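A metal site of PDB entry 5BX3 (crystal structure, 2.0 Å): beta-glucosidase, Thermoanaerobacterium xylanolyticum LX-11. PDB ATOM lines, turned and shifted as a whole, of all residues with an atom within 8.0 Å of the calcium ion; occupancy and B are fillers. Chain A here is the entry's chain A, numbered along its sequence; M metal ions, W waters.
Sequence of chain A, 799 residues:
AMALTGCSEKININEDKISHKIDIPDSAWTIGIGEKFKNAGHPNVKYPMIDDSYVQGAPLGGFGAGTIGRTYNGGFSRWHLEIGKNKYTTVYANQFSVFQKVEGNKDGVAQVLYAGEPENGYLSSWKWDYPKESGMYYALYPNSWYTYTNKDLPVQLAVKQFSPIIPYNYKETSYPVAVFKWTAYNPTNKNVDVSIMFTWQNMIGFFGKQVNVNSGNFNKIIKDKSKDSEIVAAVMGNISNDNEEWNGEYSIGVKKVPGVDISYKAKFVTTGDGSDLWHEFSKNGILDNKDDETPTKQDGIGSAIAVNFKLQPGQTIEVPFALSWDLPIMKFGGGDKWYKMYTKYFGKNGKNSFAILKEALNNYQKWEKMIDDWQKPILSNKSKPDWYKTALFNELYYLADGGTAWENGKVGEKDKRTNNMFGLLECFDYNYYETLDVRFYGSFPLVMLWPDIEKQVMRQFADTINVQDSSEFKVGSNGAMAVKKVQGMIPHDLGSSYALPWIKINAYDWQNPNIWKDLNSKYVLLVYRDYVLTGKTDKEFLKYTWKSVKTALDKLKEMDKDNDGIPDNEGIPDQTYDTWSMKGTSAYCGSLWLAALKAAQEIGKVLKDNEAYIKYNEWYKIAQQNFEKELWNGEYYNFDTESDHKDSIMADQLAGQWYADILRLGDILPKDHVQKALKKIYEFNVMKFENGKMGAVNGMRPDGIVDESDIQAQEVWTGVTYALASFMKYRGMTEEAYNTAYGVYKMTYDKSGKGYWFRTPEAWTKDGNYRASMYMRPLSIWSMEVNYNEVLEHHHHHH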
ATOM      1  N   LYS A 557      21.968  23.253   0.177  1.00  0.00           N
ATOM      2  CA  LYS A 557      20.854  22.759   1.019  1.00  0.00           C
ATOM      3  C   LYS A 557      20.032  23.892   1.650  1.00  0.00           C
ATOM      4  O   LYS A 557      18.806  23.772   1.768  1.00  0.00           O
ATOM      5  CB  LYS A 557      21.399  21.847   2.118  1.00  0.00           C
ATOM      6  CG  LYS A 557      20.367  21.134   2.988  1.00  0.00           C
ATOM      7  CD  LYS A 557      19.469  20.235   2.169  1.00  0.00           C
ATOM      8  CE  LYS A 557      18.894  19.077   2.952  1.00  0.00           C
ATOM      9  NZ  LYS A 557      17.915  19.513   3.972  1.00  0.00           N
ATOM     10  N   MET A 559      19.134  26.476   0.243  1.00  0.00           N
ATOM     11  CA  MET A 559      18.191  26.977  -0.760  1.00  0.00           C
ATOM     12  C   MET A 559      16.950  26.108  -0.932  1.00  0.00           C
ATOM     13  O   MET A 559      16.111  26.369  -1.793  1.00  0.00           O
ATOM     14  CB  MET A 559      18.906  27.190  -2.088  1.00  0.00           C
ATOM     15  CG  MET A 559      19.951  28.284  -1.968  1.00  0.00           C
ATOM     16  SD  MET A 559      20.911  28.545  -3.459  1.00  0.00           S
ATOM     17  CE  MET A 559      22.239  29.549  -2.796  1.00  0.00           C
ATOM     18  N   ASP A 560      16.804  25.082  -0.100  1.00  0.00           N
ATOM     19  CA  ASP A 560      15.576  24.302  -0.054  1.00  0.00           C
ATOM     20  C   ASP A 560      14.565  25.088   0.789  1.00  0.00           C
ATOM     21  O   ASP A 560      14.582  24.981   1.992  1.00  0.00           O
ATOM     22  CB  ASP A 560      15.844  22.922   0.536  1.00  0.00           C
ATOM     23  CG  ASP A 560      14.572  22.112   0.764  1.00  0.00           C
ATOM     24  OD1 ASP A 560      13.541  22.359   0.103  1.00  0.00           O
ATOM     25  OD2 ASP A 560      14.615  21.204   1.604  1.00  0.00           O
ATOM     26  N   LYS A 561      13.707  25.864   0.139  1.00  0.00           N
ATOM     27  CA  LYS A 561      12.712  26.701   0.837  1.00  0.00           C
ATOM     28  C   LYS A 561      11.539  25.937   1.420  1.00  0.00           C
ATOM     29  O   LYS A 561      10.935  26.423   2.379  1.00  0.00           O
ATOM     30  CB  LYS A 561      12.085  27.718  -0.114  1.00  0.00           C
ATOM     31  CG  LYS A 561      13.003  28.705  -0.792  1.00  0.00           C
ATOM     32  CD  LYS A 561      12.367  29.125  -2.116  1.00  0.00           C
ATOM     33  CE  LYS A 561      12.978  30.405  -2.667  1.00  0.00           C
ATOM     34  NZ  LYS A 561      12.376  31.621  -2.049  1.00  0.00           N
ATOM     35  N   ASP A 562      11.170  24.803   0.840  1.00  0.00           N
ATOM     36  CA  ASP A 562       9.886  24.152   1.174  1.00  0.00           C
ATOM     37  C   ASP A 562      10.057  22.793   1.838  1.00  0.00           C
ATOM     38  O   ASP A 562       9.128  21.997   1.868  1.00  0.00           O
ATOM     39  CB  ASP A 562       9.028  23.999  -0.070  1.00  0.00           C
ATOM     40  CG  ASP A 562       9.633  23.054  -1.087  1.00  0.00           C
ATOM     41  OD1 ASP A 562      10.855  22.766  -1.012  1.00  0.00           O
ATOM     42  OD2 ASP A 562       8.885  22.584  -1.956  1.00  0.00           O
ATOM     43  N   ASN A 563      11.257  22.544   2.340  1.00  0.00           N
ATOM     44  CA  ASN A 563      11.591  21.340   3.082  1.00  0.00           C
ATOM     45  C   ASN A 563      11.303  19.975   2.394  1.00  0.00           C
ATOM     46  O   ASN A 563      10.937  19.006   3.064  1.00  0.00           O
ATOM     47  CB  ASN A 563      10.939  21.380   4.484  1.00  0.00           C
ATOM     48  CG  ASN A 563      11.728  20.565   5.516  1.00  0.00           C
ATOM     49  OD1 ASN A 563      12.950  20.479   5.451  1.00  0.00           O
ATOM     50  ND2 ASN A 563      11.008  19.971   6.460  1.00  0.00           N
ATOM     51  N   ASP A 564      11.476  19.906   1.077  1.00  0.00           N
ATOM     52  CA  ASP A 564      11.402  18.611   0.380  1.00  0.00           C
ATOM     53  C   ASP A 564      12.804  17.984   0.214  1.00  0.00           C
ATOM     54  O   ASP A 564      12.936  16.905  -0.370  1.00  0.00           O
ATOM     55  CB  ASP A 564      10.657  18.737  -0.950  1.00  0.00           C
ATOM     56  CG  ASP A 564      11.436  19.521  -2.007  1.00  0.00           C
ATOM     57  OD1 ASP A 564      12.476  20.128  -1.689  1.00  0.00           O
ATOM     58  OD2 ASP A 564      10.997  19.537  -3.175  1.00  0.00           O
ATOM     59  N   GLY A 565      13.834  18.651   0.750  1.00  0.00           N
ATOM     60  CA  GLY A 565      15.198  18.155   0.726  1.00  0.00           C
ATOM     61  C   GLY A 565      15.981  18.491  -0.560  1.00  0.00           C
ATOM     62  O   GLY A 565      17.082  17.997  -0.754  1.00  0.00           O
ATOM     63  N   ILE A 566      15.403  19.342  -1.395  1.00  0.00           N
ATOM     64  CA  ILE A 566      15.971  19.680  -2.705  1.00  0.00           C
ATOM     65  C   ILE A 566      16.028  21.205  -2.848  1.00  0.00           C
ATOM     66  O   ILE A 566      15.047  21.884  -2.561  1.00  0.00           O
ATOM     67  CB  ILE A 566      15.090  19.105  -3.841  1.00  0.00           C
ATOM     68  CG1 ILE A 566      14.852  17.600  -3.653  1.00  0.00           C
ATOM     69  CG2 ILE A 566      15.698  19.357  -5.230  1.00  0.00           C
ATOM     70  CD1 ILE A 566      13.847  17.034  -4.624  1.00  0.00           C
ATOM     71  N   PRO A 567      17.167  21.762  -3.304  1.00  0.00           N
ATOM     72  CA  PRO A 567      17.139  23.203  -3.580  1.00  0.00           C
ATOM     73  C   PRO A 567      16.013  23.614  -4.539  1.00  0.00           C
ATOM     74  O   PRO A 567      15.730  22.881  -5.478  1.00  0.00           O
ATOM     75  CB  PRO A 567      18.520  23.492  -4.171  1.00  0.00           C
ATOM     76  CG  PRO A 567      19.064  22.157  -4.613  1.00  0.00           C
ATOM     77  CD  PRO A 567      18.445  21.143  -3.685  1.00  0.00           C
ATOM     78  N   ASP A 568      15.370  24.761  -4.291  1.00  0.00           N
ATOM     79  CA  ASP A 568      14.247  25.271  -5.101  1.00  0.00           C
ATOM     80  C   ASP A 568      14.733  26.309  -6.109  1.00  0.00           C
ATOM     81  O   ASP A 568      15.333  27.296  -5.708  1.00  0.00           O
ATOM     82  CB  ASP A 568      13.226  26.014  -4.225  1.00  0.00           C
ATOM     83  CG  ASP A 568      12.389  25.092  -3.344  1.00  0.00           C
ATOM     84  OD1 ASP A 568      12.973  24.395  -2.482  1.00  0.00           O
ATOM     85  OD2 ASP A 568      11.151  25.098  -3.529  1.00  0.00           O
ATOM     86  N   ASN A 569      14.437  26.114  -7.389  1.00  0.00           N
ATOM     87  CA  ASN A 569      14.649  27.148  -8.383  1.00  0.00           C
ATOM     88  C   ASN A 569      13.638  28.284  -8.098  1.00  0.00           C
ATOM     89  O   ASN A 569      12.508  28.035  -7.661  1.00  0.00           O
ATOM     90  CB  ASN A 569      14.500  26.563  -9.789  1.00  0.00           C
ATOM     91  CG  ASN A 569      15.594  25.539 -10.118  1.00  0.00           C
ATOM     92  OD1 ASN A 569      15.423  24.327  -9.939  1.00  0.00           O
ATOM     93  ND2 ASN A 569      16.718  26.026 -10.593  1.00  0.00           N
ATOM     94  N   GLY A 584      10.593  25.876  -8.492  1.00  0.00           N
ATOM     95  CA  GLY A 584      10.325  24.718  -7.642  1.00  0.00           C
ATOM     96  C   GLY A 584      11.426  23.689  -7.757  1.00  0.00           C
ATOM     97  O   GLY A 584      12.614  24.023  -7.820  1.00  0.00           O
ATOM     98  N   THR A 585      11.042  22.422  -7.821  1.00  0.00           N
ATOM     99  CA  THR A 585      12.023  21.364  -8.040  1.00  0.00           C
ATOM    100  C   THR A 585      12.101  21.168  -9.551  1.00  0.00           C
ATOM    101  O   THR A 585      11.066  20.963 -10.184  1.00  0.00           O
ATOM    102  CB  THR A 585      11.600  20.080  -7.333  1.00  0.00           C
ATOM    103  OG1 THR A 585      11.737  20.246  -5.908  1.00  0.00           O
ATOM    104  CG2 THR A 585      12.490  18.925  -7.776  1.00  0.00           C
ATOM    105  N   TRP A 593      21.643  17.563  -8.118  1.00  0.00           N
ATOM    106  CA  TRP A 593      21.706  17.533  -6.657  1.00  0.00           C
ATOM    107  C   TRP A 593      21.765  16.099  -6.143  1.00  0.00           C
ATOM    108  O   TRP A 593      22.580  15.775  -5.288  1.00  0.00           O
ATOM    109  CB  TRP A 593      20.505  18.310  -6.083  1.00  0.00           C
ATOM    110  CG  TRP A 593      20.262  18.231  -4.597  1.00  0.00           C
ATOM    111  CD1 TRP A 593      19.181  17.667  -4.007  1.00  0.00           C
ATOM    112  CD2 TRP A 593      21.076  18.750  -3.550  1.00  0.00           C
ATOM    113  NE1 TRP A 593      19.265  17.794  -2.644  1.00  0.00           N
ATOM    114  CE2 TRP A 593      20.418  18.458  -2.340  1.00  0.00           C
ATOM    115  CE3 TRP A 593      22.287  19.432  -3.512  1.00  0.00           C
ATOM    116  CZ2 TRP A 593      20.948  18.819  -1.093  1.00  0.00           C
ATOM    117  CZ3 TRP A 593      22.827  19.785  -2.278  1.00  0.00           C
ATOM    118  CH2 TRP A 593      22.142  19.480  -1.073  1.00  0.00           C
ATOM    119  N   ASN A 626      11.396  12.333  -2.929  1.00  0.00           N
ATOM    120  CA  ASN A 626      10.597  13.481  -3.324  1.00  0.00           C
ATOM    121  C   ASN A 626      10.741  13.878  -4.790  1.00  0.00           C
ATOM    122  O   ASN A 626       9.755  14.272  -5.416  1.00  0.00           O
ATOM    123  CB  ASN A 626      10.858  14.658  -2.391  1.00  0.00           C
ATOM    124  CG  ASN A 626      10.292  14.403  -1.000  1.00  0.00           C
ATOM    125  OD1 ASN A 626       9.400  13.595  -0.857  1.00  0.00           O
ATOM    126  ND2 ASN A 626      10.842  15.036   0.009  1.00  0.00           N
ATOM    127  N   GLU A 630       7.555  14.067  -7.101  1.00  0.00           N
ATOM    128  CA  GLU A 630       7.206  15.365  -7.655  1.00  0.00           C
ATOM    129  C   GLU A 630       7.231  15.437  -9.170  1.00  0.00           C
ATOM    130  O   GLU A 630       6.470  16.201  -9.758  1.00  0.00           O
ATOM    131  CB  GLU A 630       8.144  16.448  -7.102  1.00  0.00           C
ATOM    132  CG  GLU A 630       7.943  16.784  -5.628  1.00  0.00           C
ATOM    133  CD  GLU A 630       9.097  17.584  -5.037  1.00  0.00           C
ATOM    134  OE1 GLU A 630       9.970  18.070  -5.798  1.00  0.00           O
ATOM    135  OE2 GLU A 630       9.160  17.706  -3.790  1.00  0.00           O
ATOM    136  N   THR A 641       8.291  21.739 -11.095  1.00  0.00           N
ATOM    137  CA  THR A 641       7.016  21.584 -10.385  1.00  0.00           C
ATOM    138  C   THR A 641       6.113  22.814 -10.415  1.00  0.00           C
ATOM    139  O   THR A 641       4.939  22.691 -10.091  1.00  0.00           O
ATOM    140  CB  THR A 641       7.252  21.209  -8.922  1.00  0.00           C
ATOM    141  OG1 THR A 641       8.135  22.170  -8.323  1.00  0.00           O
ATOM    142  CG2 THR A 641       7.864  19.817  -8.816  1.00  0.00           C
ATOM    143  N   GLU A 642       6.623  23.981 -10.776  1.00  0.00           N
ATOM    144  CA  GLU A 642       5.828  25.226 -10.656  1.00  0.00           C
ATOM    145  C   GLU A 642       5.765  26.166 -11.876  1.00  0.00           C
ATOM    146  O   GLU A 642       4.996  27.105 -11.852  1.00  0.00           O
ATOM    147  CB  GLU A 642       6.281  26.027  -9.435  1.00  0.00           C
ATOM    148  CG  GLU A 642       6.099  25.286  -8.107  1.00  0.00           C
ATOM    149  CD  GLU A 642       6.653  26.055  -6.928  1.00  0.00           C
ATOM    150  OE1 GLU A 642       6.663  27.305  -6.986  1.00  0.00           O
ATOM    151  OE2 GLU A 642       7.076  25.424  -5.931  1.00  0.00           O
HETATM  152 CA    CA M   1      12.873  22.210  -2.046  1.00  0.00          CA
HETATM  153  O   HOH W   1      12.992  22.131  -4.463  1.00  0.00           O
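Of the 19 residues printed, 5 come within 4 Å of the calcium ion. Along chain A the residues within 4 Å of the calcium ion span positions 560 to 568. The nearest printed residue that does not touch the calcium ion is Pro 567 (4.2 Å).
The side-chain hydroxyl (OG1) of Thr 585 is in hydrogen-bond range of the side-chain carboxylate (OD2) of Asp 564, 2.9 Å away. The side-chain carboxylate of Glu 630 lies close to the side-chain carboxylate of Asp 564, 2.7 Å away. The side-chain amide nitrogen (ND2) of Asn 626 lies within hydrogen-bond range of the backbone carbonyl oxygen (O) of Asp 564 (2.8 Å). N of Lys 561 sits close to OD1 of Asp 568 (3.1 Å). The backbone NH (N) of Asp 568 lies within hydrogen-bond range of the backbone carbonyl oxygen (O) of Met 559, at 3.1 Å. N of Gly 565 sits at hydrogen-bond distance from OD2 of Asp 560 (2.8 Å). OD1 of Asp 560 lies close to N of Asn 563 (3.2 Å).
Water W1 lies within hydrogen-bond range of OG1 of Thr 585 and O of Pro 567.
The calcium ion is bound by OD1 of Asp 564 (2.1 Å), OD1 of Asp 568 (2.2 Å), OD1 of Asp 560 (2.3 Å), O of Ile 566 (2.3 Å), OD1 of Asp 562 (2.3 Å) and water W1 (2.4 Å). The calcium ion has six donor atoms within binding distance.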
